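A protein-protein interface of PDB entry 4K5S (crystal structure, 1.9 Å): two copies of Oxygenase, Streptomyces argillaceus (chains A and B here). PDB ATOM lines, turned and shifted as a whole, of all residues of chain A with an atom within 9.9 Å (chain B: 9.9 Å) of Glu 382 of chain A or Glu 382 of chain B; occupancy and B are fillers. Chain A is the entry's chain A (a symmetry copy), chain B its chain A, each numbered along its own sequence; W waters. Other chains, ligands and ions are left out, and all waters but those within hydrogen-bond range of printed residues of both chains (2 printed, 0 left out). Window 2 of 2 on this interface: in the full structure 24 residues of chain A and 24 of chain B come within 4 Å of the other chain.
The side-chain carboxylate (OE1) of Glu 376 of chain B lies within hydrogen-bond range of the side-chain hydroxyl (OH) of Tyr 386 of chain A (2.6 Å). OE1 of Glu 376 of chain A sits at hydrogen-bond distance from OH of Tyr 386 of chain B (2.6 Å).
The side-chain hydroxyl of Thr 380 of chain B sits at hydrogen-bond distance from the backbone carbonyl oxygen of Leu 377 of chain B. The side-chain hydroxyl (OG1) of Thr 380 of chain A is in hydrogen-bond range of the backbone carbonyl oxygen (O) of Leu 377 of chain A (2.6 Å).
Leu 377 of chain A touches Tyr 386 of chain B (CD2 to CD2, 3.7 Å). Glu 382 of chain B touches Glu 382 of chain A (OE2 to CB, 3.2 Å). Val 383 of chain A touches Val 383 of chain B (CG2 to CG2, 3.4 Å). Leu 377 of chain B touches Tyr 386 of chain A (CD2 to CD2, 3.7 Å).
Of the printed residues of chain B, Glu 376 of chain A touches Tyr 386 (2.6 Å). Printed residues of chain B within 4 Å of Leu 377 of chain A: Tyr 386 (3.7 Å). Gly 379 of chain A touches none of the printed residues of chain B. No residue of chain B comes within 4 Å of Thr 380 of chain A. No residue of chain B comes within 4 Å of Asp 381 of chain A. Of chain B, only Glu 382 comes within 4 Å of Glu 382 of chain A. Printed residues of chain B within 4 Å of Tyr 386 of chain A: Glu 376 and Leu 377. Asp 97 of chain B touches none of the printed residues of chain A. No residue of chain A comes within 4 Å of Thr 380 of chain B. No residue of chain A comes within 4 Å of Asp 381 of chain B. Arg 385 of chain B touches none of the printed residues of chain A.
Hydrophobic or aromatic side chains of chain B that line the printed part of chain A: Leu 377, Val 383 and Tyr 386. Printed residues of chain A that touch a printed residue of chain B: Glu 376, Leu 377, Glu 382, Val 383 and Tyr 386. Hydrophobic or aromatic side chains of chain A within 4 Å of the printed part of chain B: Leu 377, Val 383 and Tyr 386. Among the printed residues, 6 pairs touch across the chains. Among the printed residues, no Asp or Glu carboxylate lies within 4 Å of a Lys or Arg side-chain nitrogen of the other chain.
Glu 376 of chain A touches Tyr 386 of chain B, and with the chains exchanged Tyr 386 of chain A touches Glu 376 of chain B. Leu 377 of chain A touches Tyr 386 of chain B, and with the chains exchanged Tyr 386 of chain A touches Leu 377 of chain B. Glu 382 of chain B touches its own counterpart, Glu 382 of chain A. Val 383 of chain A touches its own counterpart, Val 383 of chain B. Of the 6 pairs that touch across the chains among the printed residues, 6 have their exchanged pair printed and touching as well.
Water W1 lies within hydrogen-bond range of the side-chain carboxylate of Glu 382 of chain A, the backbone NH of Glu 382 of chain B and the backbone NH of Asp 381 of chain B. Water W2 lies within hydrogen-bond range of OE2 of Glu 382 of chain B (2.5 Å), N of Glu 382 of chain A (2.8 Å) and N of Asp 381 of chain A (3.3 Å).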
ATOM      1  N   LEU A  96     -29.466 -13.041  14.804  1.00  0.00           N
ATOM      2  CA  LEU A  96     -29.775 -14.186  13.973  1.00  0.00           C
ATOM      3  C   LEU A  96     -31.250 -14.524  14.139  1.00  0.00           C
ATOM      4  O   LEU A  96     -31.756 -14.620  15.263  1.00  0.00           O
ATOM      5  CB  LEU A  96     -28.888 -15.366  14.350  1.00  0.00           C
ATOM      6  CG  LEU A  96     -27.394 -15.037  14.271  1.00  0.00           C
ATOM      7  CD1 LEU A  96     -26.577 -16.263  14.645  1.00  0.00           C
ATOM      8  CD2 LEU A  96     -26.996 -14.519  12.875  1.00  0.00           C
ATOM      9  N   ASP A  97     -31.942 -14.690  13.018  1.00  0.00           N
ATOM     10  CA  ASP A  97     -33.394 -14.805  13.040  1.00  0.00           C
ATOM     11  C   ASP A  97     -33.852 -16.259  12.861  1.00  0.00           C
ATOM     12  O   ASP A  97     -33.842 -16.788  11.747  1.00  0.00           O
ATOM     13  CB  ASP A  97     -33.979 -13.918  11.939  1.00  0.00           C
ATOM     14  CG  ASP A  97     -35.494 -13.909  11.931  1.00  0.00           C
ATOM     15  OD1 ASP A  97     -36.116 -14.733  12.637  1.00  0.00           O
ATOM     16  OD2 ASP A  97     -36.062 -13.076  11.194  1.00  0.00           O
ATOM     17  N   LEU A 100     -36.161 -17.720   9.994  1.00  0.00           N
ATOM     18  CA  LEU A 100     -35.740 -17.839   8.593  1.00  0.00           C
ATOM     19  C   LEU A 100     -35.236 -19.234   8.281  1.00  0.00           C
ATOM     20  O   LEU A 100     -34.852 -19.532   7.146  1.00  0.00           O
ATOM     21  CB  LEU A 100     -34.624 -16.838   8.281  1.00  0.00           C
ATOM     22  CG  LEU A 100     -34.961 -15.352   8.381  1.00  0.00           C
ATOM     23  CD1 LEU A 100     -33.712 -14.497   8.141  1.00  0.00           C
ATOM     24  CD2 LEU A 100     -36.070 -15.004   7.392  1.00  0.00           C
ATOM     25  N   VAL A 101     -35.199 -20.082   9.299  1.00  0.00           N
ATOM     26  CA  VAL A 101     -34.766 -21.447   9.087  1.00  0.00           C
ATOM     27  C   VAL A 101     -35.891 -22.415   9.425  1.00  0.00           C
ATOM     28  O   VAL A 101     -36.814 -22.079  10.166  1.00  0.00           O
ATOM     29  CB  VAL A 101     -33.464 -21.778   9.849  1.00  0.00           C
ATOM     30  CG1 VAL A 101     -32.279 -20.998   9.248  1.00  0.00           C
ATOM     31  CG2 VAL A 101     -33.617 -21.498  11.337  1.00  0.00           C
ATOM     32  N   GLU A 376     -25.629  -4.128   8.452  1.00  0.00           N
ATOM     33  CA  GLU A 376     -26.629  -3.888   7.414  1.00  0.00           C
ATOM     34  C   GLU A 376     -27.020  -5.192   6.737  1.00  0.00           C
ATOM     35  O   GLU A 376     -28.201  -5.476   6.549  1.00  0.00           O
ATOM     36  CB  GLU A 376     -26.093  -2.961   6.320  1.00  0.00           C
ATOM     37  CG  GLU A 376     -26.146  -1.480   6.608  1.00  0.00           C
ATOM     38  CD  GLU A 376     -25.610  -0.651   5.441  1.00  0.00           C
ATOM     39  OE1 GLU A 376     -25.811  -1.060   4.276  1.00  0.00           O
ATOM     40  OE2 GLU A 376     -24.962   0.392   5.692  1.00  0.00           O
ATOM     41  N   LEU A 377     -26.018  -5.965   6.340  1.00  0.00           N
ATOM     42  CA  LEU A 377     -26.255  -7.211   5.624  1.00  0.00           C
ATOM     43  C   LEU A 377     -27.047  -8.201   6.461  1.00  0.00           C
ATOM     44  O   LEU A 377     -27.829  -8.977   5.922  1.00  0.00           O
ATOM     45  CB  LEU A 377     -24.941  -7.843   5.173  1.00  0.00           C
ATOM     46  CG  LEU A 377     -24.282  -7.079   4.026  1.00  0.00           C
ATOM     47  CD1 LEU A 377     -22.922  -7.664   3.685  1.00  0.00           C
ATOM     48  CD2 LEU A 377     -25.197  -7.071   2.817  1.00  0.00           C
ATOM     49  N   LEU A 378     -26.830  -8.177   7.773  1.00  0.00           N
ATOM     50  CA  LEU A 378     -27.572  -9.043   8.685  1.00  0.00           C
ATOM     51  C   LEU A 378     -29.068  -8.725   8.717  1.00  0.00           C
ATOM     52  O   LEU A 378     -29.877  -9.552   9.144  1.00  0.00           O
ATOM     53  CB  LEU A 378     -26.983  -8.972  10.099  1.00  0.00           C
ATOM     54  CG  LEU A 378     -25.670  -9.742  10.280  1.00  0.00           C
ATOM     55  CD1 LEU A 378     -24.956  -9.347  11.579  1.00  0.00           C
ATOM     56  CD2 LEU A 378     -25.881 -11.271  10.195  1.00  0.00           C
ATOM     57  N   GLY A 379     -29.436  -7.527   8.277  1.00  0.00           N
ATOM     58  CA  GLY A 379     -30.838  -7.158   8.177  1.00  0.00           C
ATOM     59  C   GLY A 379     -31.483  -7.600   6.872  1.00  0.00           C
ATOM     60  O   GLY A 379     -32.634  -7.269   6.598  1.00  0.00           O
ATOM     61  N   THR A 380     -30.741  -8.330   6.046  1.00  0.00           N
ATOM     62  CA  THR A 380     -31.341  -8.944   4.868  1.00  0.00           C
ATOM     63  C   THR A 380     -31.570 -10.418   5.166  1.00  0.00           C
ATOM     64  O   THR A 380     -30.753 -11.061   5.836  1.00  0.00           O
ATOM     65  CB  THR A 380     -30.465  -8.801   3.598  1.00  0.00           C
ATOM     66  OG1 THR A 380     -29.241  -9.527   3.774  1.00  0.00           O
ATOM     67  CG2 THR A 380     -30.158  -7.336   3.316  1.00  0.00           C
ATOM     68  N   ASP A 381     -32.690 -10.947   4.684  1.00  0.00           N
ATOM     69  CA  ASP A 381     -33.076 -12.316   4.991  1.00  0.00           C
ATOM     70  C   ASP A 381     -32.021 -13.300   4.522  1.00  0.00           C
ATOM     71  O   ASP A 381     -31.677 -14.226   5.241  1.00  0.00           O
ATOM     72  CB  ASP A 381     -34.428 -12.653   4.367  1.00  0.00           C
ATOM     73  CG  ASP A 381     -35.587 -12.083   5.153  1.00  0.00           C
ATOM     74  OD1 ASP A 381     -35.347 -11.352   6.142  1.00  0.00           O
ATOM     75  OD2 ASP A 381     -36.741 -12.361   4.774  1.00  0.00           O
ATOM     76  N   GLU A 382     -31.498 -13.091   3.320  1.00  0.00           N
ATOM     77  CA  GLU A 382     -30.546 -14.040   2.745  1.00  0.00           C
ATOM     78  C   GLU A 382     -29.243 -14.173   3.542  1.00  0.00           C
ATOM     79  O   GLU A 382     -28.779 -15.281   3.813  1.00  0.00           O
ATOM     80  CB  GLU A 382     -30.243 -13.691   1.285  1.00  0.00           C
ATOM     81  CG  GLU A 382     -30.714 -14.748   0.305  1.00  0.00           C
ATOM     82  CD  GLU A 382     -29.741 -14.952  -0.845  1.00  0.00           C
ATOM     83  OE1 GLU A 382     -29.383 -16.118  -1.126  1.00  0.00           O
ATOM     84  OE2 GLU A 382     -29.337 -13.947  -1.468  1.00  0.00           O
ATOM     85  N   VAL A 383     -28.644 -13.052   3.913  1.00  0.00           N
ATOM     86  CA  VAL A 383     -27.419 -13.120   4.691  1.00  0.00           C
ATOM     87  C   VAL A 383     -27.700 -13.589   6.118  1.00  0.00           C
ATOM     88  O   VAL A 383     -26.938 -14.376   6.682  1.00  0.00           O
ATOM     89  CB  VAL A 383     -26.674 -11.782   4.695  1.00  0.00           C
ATOM     90  CG1 VAL A 383     -25.448 -11.851   5.590  1.00  0.00           C
ATOM     91  CG2 VAL A 383     -26.276 -11.406   3.266  1.00  0.00           C
ATOM     92  N   ASN A 384     -28.793 -13.114   6.706  1.00  0.00           N
ATOM     93  CA  ASN A 384     -29.125 -13.540   8.059  1.00  0.00           C
ATOM     94  C   ASN A 384     -29.373 -15.048   8.092  1.00  0.00           C
ATOM     95  O   ASN A 384     -28.937 -15.745   9.015  1.00  0.00           O
ATOM     96  CB  ASN A 384     -30.330 -12.778   8.594  1.00  0.00           C
ATOM     97  CG  ASN A 384     -30.524 -12.977  10.085  1.00  0.00           C
ATOM     98  OD1 ASN A 384     -30.856 -14.068  10.535  1.00  0.00           O
ATOM     99  ND2 ASN A 384     -30.316 -11.920  10.857  1.00  0.00           N
ATOM    100  N   ARG A 385     -30.041 -15.557   7.063  1.00  0.00           N
ATOM    101  CA  ARG A 385     -30.312 -16.988   6.985  1.00  0.00           C
ATOM    102  C   ARG A 385     -29.008 -17.789   6.919  1.00  0.00           C
ATOM    103  O   ARG A 385     -28.868 -18.838   7.539  1.00  0.00           O
ATOM    104  CB  ARG A 385     -31.179 -17.296   5.764  1.00  0.00           C
ATOM    105  CG  ARG A 385     -31.605 -18.750   5.680  1.00  0.00           C
ATOM    106  CD  ARG A 385     -32.637 -18.965   4.571  1.00  0.00           C
ATOM    107  NE  ARG A 385     -33.890 -18.235   4.794  1.00  0.00           N
ATOM    108  CZ  ARG A 385     -34.314 -17.217   4.046  1.00  0.00           C
ATOM    109  NH1 ARG A 385     -33.590 -16.788   3.016  1.00  0.00           N
ATOM    110  NH2 ARG A 385     -35.469 -16.626   4.323  1.00  0.00           N
ATOM    111  N   TYR A 386     -28.063 -17.270   6.152  1.00  0.00           N
ATOM    112  CA  TYR A 386     -26.734 -17.855   5.990  1.00  0.00           C
ATOM    113  C   TYR A 386     -26.003 -18.011   7.322  1.00  0.00           C
ATOM    114  O   TYR A 386     -25.513 -19.091   7.660  1.00  0.00           O
ATOM    115  CB  TYR A 386     -25.929 -16.943   5.050  1.00  0.00           C
ATOM    116  CG  TYR A 386     -24.508 -17.363   4.764  1.00  0.00           C
ATOM    117  CD1 TYR A 386     -24.227 -18.391   3.861  1.00  0.00           C
ATOM    118  CD2 TYR A 386     -23.443 -16.705   5.364  1.00  0.00           C
ATOM    119  CE1 TYR A 386     -22.927 -18.759   3.589  1.00  0.00           C
ATOM    120  CE2 TYR A 386     -22.135 -17.066   5.096  1.00  0.00           C
ATOM    121  CZ  TYR A 386     -21.884 -18.088   4.210  1.00  0.00           C
ATOM    122  OH  TYR A 386     -20.585 -18.440   3.949  1.00  0.00           O
ATOM    123  N   PHE A 387     -25.916 -16.932   8.085  1.00  0.00           N
ATOM    124  CA  PHE A 387     -25.189 -17.001   9.343  1.00  0.00           C
ATOM    125  C   PHE A 387     -25.969 -17.748  10.416  1.00  0.00           C
ATOM    126  O   PHE A 387     -25.379 -18.432  11.241  1.00  0.00           O
ATOM    127  CB  PHE A 387     -24.731 -15.619   9.799  1.00  0.00           C
ATOM    128  CG  PHE A 387     -23.606 -15.068   8.962  1.00  0.00           C
ATOM    129  CD1 PHE A 387     -22.396 -15.745   8.875  1.00  0.00           C
ATOM    130  CD2 PHE A 387     -23.764 -13.890   8.245  1.00  0.00           C
ATOM    131  CE1 PHE A 387     -21.344 -15.244   8.095  1.00  0.00           C
ATOM    132  CE2 PHE A 387     -22.728 -13.386   7.466  1.00  0.00           C
ATOM    133  CZ  PHE A 387     -21.514 -14.061   7.390  1.00  0.00           C
ATOM    134  N   THR A 388     -27.292 -17.655  10.377  1.00  0.00           N
ATOM    135  CA  THR A 388     -28.109 -18.420  11.308  1.00  0.00           C
ATOM    136  C   THR A 388     -27.936 -19.925  11.101  1.00  0.00           C
ATOM    137  O   THR A 388     -27.746 -20.672  12.064  1.00  0.00           O
ATOM    138  CB  THR A 388     -29.589 -18.046  11.193  1.00  0.00           C
ATOM    139  OG1 THR A 388     -29.748 -16.660  11.517  1.00  0.00           O
ATOM    140  CG2 THR A 388     -30.419 -18.877  12.153  1.00  0.00           C
ATOM    141  N   GLY A 389     -27.980 -20.360   9.845  1.00  0.00           N
ATOM    142  CA  GLY A 389     -27.791 -21.760   9.514  1.00  0.00           C
ATOM    143  C   GLY A 389     -26.411 -22.253   9.914  1.00  0.00           C
ATOM    144  O   GLY A 389     -26.237 -23.397  10.346  1.00  0.00           O
ATOM    145  N   MET A 390     -25.423 -21.379   9.760  1.00  0.00           N
ATOM    146  CA  MET A 390     -24.041 -21.688  10.108  1.00  0.00           C
ATOM    147  C   MET A 390     -23.879 -21.939  11.610  1.00  0.00           C
ATOM    148  O   MET A 390     -23.331 -22.962  12.035  1.00  0.00           O
ATOM    149  CB  MET A 390     -23.144 -20.531   9.677  1.00  0.00           C
ATOM    150  CG  MET A 390     -21.652 -20.750   9.879  1.00  0.00           C
ATOM    151  SD  MET A 390     -20.699 -19.320   9.309  1.00  0.00           S
ATOM    152  CE  MET A 390     -20.704 -18.305  10.775  1.00  0.00           C
ATOM    153  N   LEU B  96     -17.516  -8.477  -9.128  1.00  0.00           N
ATOM    154  CA  LEU B  96     -18.749  -7.718  -9.141  1.00  0.00           C
ATOM    155  C   LEU B  96     -19.431  -7.920 -10.487  1.00  0.00           C
ATOM    156  O   LEU B  96     -18.800  -7.792 -11.542  1.00  0.00           O
ATOM    157  CB  LEU B  96     -18.464  -6.245  -8.877  1.00  0.00           C
ATOM    158  CG  LEU B  96     -17.706  -6.011  -7.566  1.00  0.00           C
ATOM    159  CD1 LEU B  96     -17.473  -4.522  -7.365  1.00  0.00           C
ATOM    160  CD2 LEU B  96     -18.451  -6.615  -6.359  1.00  0.00           C
ATOM    161  N   ASP B  97     -20.717  -8.248 -10.447  1.00  0.00           N
ATOM    162  CA  ASP B  97     -21.422  -8.672 -11.650  1.00  0.00           C
ATOM    163  C   ASP B  97     -22.315  -7.557 -12.209  1.00  0.00           C
ATOM    164  O   ASP B  97     -23.399  -7.296 -11.683  1.00  0.00           O
ATOM    165  CB  ASP B  97     -22.254  -9.915 -11.324  1.00  0.00           C
ATOM    166  CG  ASP B  97     -22.968 -10.481 -12.535  1.00  0.00           C
ATOM    167  OD1 ASP B  97     -22.995  -9.819 -13.596  1.00  0.00           O
ATOM    168  OD2 ASP B  97     -23.520 -11.594 -12.411  1.00  0.00           O
ATOM    169  N   LEU B 100     -26.237  -7.654 -12.751  1.00  0.00           N
ATOM    170  CA  LEU B 100     -27.208  -7.673 -11.652  1.00  0.00           C
ATOM    171  C   LEU B 100     -27.735  -6.284 -11.351  1.00  0.00           C
ATOM    172  O   LEU B 100     -28.576  -6.100 -10.467  1.00  0.00           O
ATOM    173  CB  LEU B 100     -26.568  -8.234 -10.379  1.00  0.00           C
ATOM    174  CG  LEU B 100     -26.101  -9.688 -10.407  1.00  0.00           C
ATOM    175  CD1 LEU B 100     -25.393 -10.054  -9.097  1.00  0.00           C
ATOM    176  CD2 LEU B 100     -27.287 -10.610 -10.673  1.00  0.00           C
ATOM    177  N   VAL B 101     -27.211  -5.296 -12.063  1.00  0.00           N
ATOM    178  CA  VAL B 101     -27.681  -3.939 -11.870  1.00  0.00           C
ATOM    179  C   VAL B 101     -28.292  -3.405 -13.158  1.00  0.00           C
ATOM    180  O   VAL B 101     -28.006  -3.901 -14.248  1.00  0.00           O
ATOM    181  CB  VAL B 101     -26.580  -3.007 -11.318  1.00  0.00           C
ATOM    182  CG1 VAL B 101     -26.221  -3.401  -9.872  1.00  0.00           C
ATOM    183  CG2 VAL B 101     -25.353  -3.019 -12.219  1.00  0.00           C
ATOM    184  N   GLU B 376     -17.547 -16.438  -0.694  1.00  0.00           N
ATOM    185  CA  GLU B 376     -18.761 -17.232  -0.868  1.00  0.00           C
ATOM    186  C   GLU B 376     -19.967 -16.328  -1.063  1.00  0.00           C
ATOM    187  O   GLU B 376     -20.776 -16.541  -1.964  1.00  0.00           O
ATOM    188  CB  GLU B 376     -19.048 -18.097   0.363  1.00  0.00           C
ATOM    189  CG  GLU B 376     -18.298 -19.404   0.456  1.00  0.00           C
ATOM    190  CD  GLU B 376     -18.680 -20.194   1.708  1.00  0.00           C
ATOM    191  OE1 GLU B 376     -19.860 -20.131   2.117  1.00  0.00           O
ATOM    192  OE2 GLU B 376     -17.791 -20.852   2.297  1.00  0.00           O
ATOM    193  N   LEU B 377     -20.101 -15.337  -0.192  1.00  0.00           N
ATOM    194  CA  LEU B 377     -21.244 -14.437  -0.231  1.00  0.00           C
ATOM    195  C   LEU B 377     -21.307 -13.661  -1.536  1.00  0.00           C
ATOM    196  O   LEU B 377     -22.392 -13.351  -2.018  1.00  0.00           O
ATOM    197  CB  LEU B 377     -21.223 -13.471   0.950  1.00  0.00           C
ATOM    198  CG  LEU B 377     -21.555 -14.153   2.276  1.00  0.00           C
ATOM    199  CD1 LEU B 377     -21.407 -13.190   3.442  1.00  0.00           C
ATOM    200  CD2 LEU B 377     -22.953 -14.739   2.220  1.00  0.00           C
ATOM    201  N   LEU B 378     -20.143 -13.339  -2.092  1.00  0.00           N
ATOM    202  CA  LEU B 378     -20.076 -12.642  -3.373  1.00  0.00           C
ATOM    203  C   LEU B 378     -20.634 -13.474  -4.529  1.00  0.00           C
ATOM    204  O   LEU B 378     -20.975 -12.934  -5.585  1.00  0.00           O
ATOM    205  CB  LEU B 378     -18.637 -12.206  -3.678  1.00  0.00           C
ATOM    206  CG  LEU B 378     -18.160 -10.988  -2.880  1.00  0.00           C
ATOM    207  CD1 LEU B 378     -16.636 -10.823  -2.954  1.00  0.00           C
ATOM    208  CD2 LEU B 378     -18.888  -9.694  -3.309  1.00  0.00           C
ATOM    209  N   GLY B 379     -20.720 -14.785  -4.338  1.00  0.00           N
ATOM    210  CA  GLY B 379     -21.322 -15.655  -5.334  1.00  0.00           C
ATOM    211  C   GLY B 379     -22.835 -15.754  -5.209  1.00  0.00           C
ATOM    212  O   GLY B 379     -23.473 -16.532  -5.914  1.00  0.00           O
ATOM    213  N   THR B 380     -23.419 -14.983  -4.297  1.00  0.00           N
ATOM    214  CA  THR B 380     -24.872 -14.883  -4.242  1.00  0.00           C
ATOM    215  C   THR B 380     -25.282 -13.569  -4.889  1.00  0.00           C
ATOM    216  O   THR B 380     -24.597 -12.550  -4.737  1.00  0.00           O
ATOM    217  CB  THR B 380     -25.429 -14.946  -2.797  1.00  0.00           C
ATOM    218  OG1 THR B 380     -24.981 -13.802  -2.059  1.00  0.00           O
ATOM    219  CG2 THR B 380     -24.974 -16.220  -2.098  1.00  0.00           C
ATOM    220  N   ASP B 381     -26.388 -13.597  -5.625  1.00  0.00           N
ATOM    221  CA  ASP B 381     -26.825 -12.434  -6.382  1.00  0.00           C
ATOM    222  C   ASP B 381     -27.069 -11.247  -5.470  1.00  0.00           C
ATOM    223  O   ASP B 381     -26.670 -10.134  -5.782  1.00  0.00           O
ATOM    224  CB  ASP B 381     -28.084 -12.750  -7.186  1.00  0.00           C
ATOM    225  CG  ASP B 381     -27.786 -13.535  -8.444  1.00  0.00           C
ATOM    226  OD1 ASP B 381     -26.610 -13.912  -8.659  1.00  0.00           O
ATOM    227  OD2 ASP B 381     -28.733 -13.782  -9.214  1.00  0.00           O
ATOM    228  N   GLU B 382     -27.712 -11.486  -4.334  1.00  0.00           N
ATOM    229  CA  GLU B 382     -28.077 -10.390  -3.437  1.00  0.00           C
ATOM    230  C   GLU B 382     -26.876  -9.630  -2.864  1.00  0.00           C
ATOM    231  O   GLU B 382     -26.847  -8.400  -2.866  1.00  0.00           O
ATOM    232  CB  GLU B 382     -28.979 -10.889  -2.306  1.00  0.00           C
ATOM    233  CG  GLU B 382     -30.377 -10.299  -2.347  1.00  0.00           C
ATOM    234  CD  GLU B 382     -30.919  -9.987  -0.962  1.00  0.00           C
ATOM    235  OE1 GLU B 382     -31.406  -8.854  -0.751  1.00  0.00           O
ATOM    236  OE2 GLU B 382     -30.861 -10.877  -0.086  1.00  0.00           O
ATOM    237  N   VAL B 383     -25.885 -10.354  -2.365  1.00  0.00           N
ATOM    238  CA  VAL B 383     -24.710  -9.685  -1.831  1.00  0.00           C
ATOM    239  C   VAL B 383     -23.868  -9.076  -2.951  1.00  0.00           C
ATOM    240  O   VAL B 383     -23.347  -7.969  -2.813  1.00  0.00           O
ATOM    241  CB  VAL B 383     -23.867 -10.626  -0.965  1.00  0.00           C
ATOM    242  CG1 VAL B 383     -22.598  -9.934  -0.497  1.00  0.00           C
ATOM    243  CG2 VAL B 383     -24.689 -11.109   0.231  1.00  0.00           C
ATOM    244  N   ASN B 384     -23.733  -9.791  -4.063  1.00  0.00           N
ATOM    245  CA  ASN B 384     -22.958  -9.254  -5.173  1.00  0.00           C
ATOM    246  C   ASN B 384     -23.602  -7.969  -5.694  1.00  0.00           C
ATOM    247  O   ASN B 384     -22.912  -6.991  -6.002  1.00  0.00           O
ATOM    248  CB  ASN B 384     -22.813 -10.282  -6.289  1.00  0.00           C
ATOM    249  CG  ASN B 384     -21.779  -9.872  -7.321  1.00  0.00           C
ATOM    250  OD1 ASN B 384     -21.974  -8.913  -8.058  1.00  0.00           O
ATOM    251  ND2 ASN B 384     -20.673 -10.600  -7.373  1.00  0.00           N
ATOM    252  N   ARG B 385     -24.929  -7.959  -5.757  1.00  0.00           N
ATOM    253  CA  ARG B 385     -25.644  -6.775  -6.218  1.00  0.00           C
ATOM    254  C   ARG B 385     -25.380  -5.581  -5.294  1.00  0.00           C
ATOM    255  O   ARG B 385     -25.202  -4.453  -5.741  1.00  0.00           O
ATOM    256  CB  ARG B 385     -27.144  -7.059  -6.292  1.00  0.00           C
ATOM    257  CG  ARG B 385     -27.945  -5.912  -6.879  1.00  0.00           C
ATOM    258  CD  ARG B 385     -29.399  -6.319  -7.131  1.00  0.00           C
ATOM    259  NE  ARG B 385     -29.539  -7.397  -8.115  1.00  0.00           N
ATOM    260  CZ  ARG B 385     -29.965  -8.628  -7.832  1.00  0.00           C
ATOM    261  NH1 ARG B 385     -30.295  -8.959  -6.587  1.00  0.00           N
ATOM    262  NH2 ARG B 385     -30.066  -9.533  -8.796  1.00  0.00           N
ATOM    263  N   TYR B 386     -25.363  -5.860  -4.001  1.00  0.00           N
ATOM    264  CA  TYR B 386     -25.085  -4.874  -2.959  1.00  0.00           C
ATOM    265  C   TYR B 386     -23.730  -4.195  -3.151  1.00  0.00           C
ATOM    266  O   TYR B 386     -23.625  -2.967  -3.164  1.00  0.00           O
ATOM    267  CB  TYR B 386     -25.128  -5.595  -1.603  1.00  0.00           C
ATOM    268  CG  TYR B 386     -24.846  -4.748  -0.386  1.00  0.00           C
ATOM    269  CD1 TYR B 386     -25.817  -3.893   0.139  1.00  0.00           C
ATOM    270  CD2 TYR B 386     -23.623  -4.835   0.266  1.00  0.00           C
ATOM    271  CE1 TYR B 386     -25.562  -3.136   1.263  1.00  0.00           C
ATOM    272  CE2 TYR B 386     -23.358  -4.080   1.394  1.00  0.00           C
ATOM    273  CZ  TYR B 386     -24.327  -3.237   1.887  1.00  0.00           C
ATOM    274  OH  TYR B 386     -24.058  -2.494   3.006  1.00  0.00           O
ATOM    275  N   PHE B 387     -22.679  -4.990  -3.291  1.00  0.00           N
ATOM    276  CA  PHE B 387     -21.354  -4.407  -3.427  1.00  0.00           C
ATOM    277  C   PHE B 387     -21.131  -3.799  -4.805  1.00  0.00           C
ATOM    278  O   PHE B 387     -20.443  -2.796  -4.931  1.00  0.00           O
ATOM    279  CB  PHE B 387     -20.265  -5.402  -3.036  1.00  0.00           C
ATOM    280  CG  PHE B 387     -20.208  -5.658  -1.552  1.00  0.00           C
ATOM    281  CD1 PHE B 387     -19.959  -4.616  -0.668  1.00  0.00           C
ATOM    282  CD2 PHE B 387     -20.425  -6.929  -1.041  1.00  0.00           C
ATOM    283  CE1 PHE B 387     -19.909  -4.841   0.715  1.00  0.00           C
ATOM    284  CE2 PHE B 387     -20.381  -7.163   0.329  1.00  0.00           C
ATOM    285  CZ  PHE B 387     -20.121  -6.120   1.211  1.00  0.00           C
ATOM    286  N   THR B 388     -21.749  -4.378  -5.827  1.00  0.00           N
ATOM    287  CA  THR B 388     -21.665  -3.797  -7.159  1.00  0.00           C
ATOM    288  C   THR B 388     -22.303  -2.407  -7.207  1.00  0.00           C
ATOM    289  O   THR B 388     -21.715  -1.466  -7.743  1.00  0.00           O
ATOM    290  CB  THR B 388     -22.313  -4.703  -8.209  1.00  0.00           C
ATOM    291  OG1 THR B 388     -21.618  -5.955  -8.239  1.00  0.00           O
ATOM    292  CG2 THR B 388     -22.236  -4.060  -9.580  1.00  0.00           C
ATOM    293  N   GLY B 389     -23.492  -2.282  -6.626  1.00  0.00           N
ATOM    294  CA  GLY B 389     -24.184  -1.007  -6.569  1.00  0.00           C
ATOM    295  C   GLY B 389     -23.397   0.028  -5.784  1.00  0.00           C
ATOM    296  O   GLY B 389     -23.388   1.218  -6.116  1.00  0.00           O
ATOM    297  N   MET B 390     -22.736  -0.434  -4.729  1.00  0.00           N
ATOM    298  CA  MET B 390     -21.923   0.424  -3.875  1.00  0.00           C
ATOM    299  C   MET B 390     -20.732   1.014  -4.638  1.00  0.00           C
ATOM    300  O   MET B 390     -20.510   2.230  -4.641  1.00  0.00           O
ATOM    301  CB  MET B 390     -21.424  -0.383  -2.680  1.00  0.00           C
ATOM    302  CG  MET B 390     -20.643   0.404  -1.639  1.00  0.00           C
ATOM    303  SD  MET B 390     -20.129  -0.659  -0.266  1.00  0.00           S
ATOM    304  CE  MET B 390     -18.581  -1.288  -0.888  1.00  0.00           C
HETATM  305  O   HOH W   1     -29.203 -13.797  -3.948  1.00  0.00           O
HETATM  306  O   HOH W   2     -32.736 -11.463   1.442  1.00  0.00           O
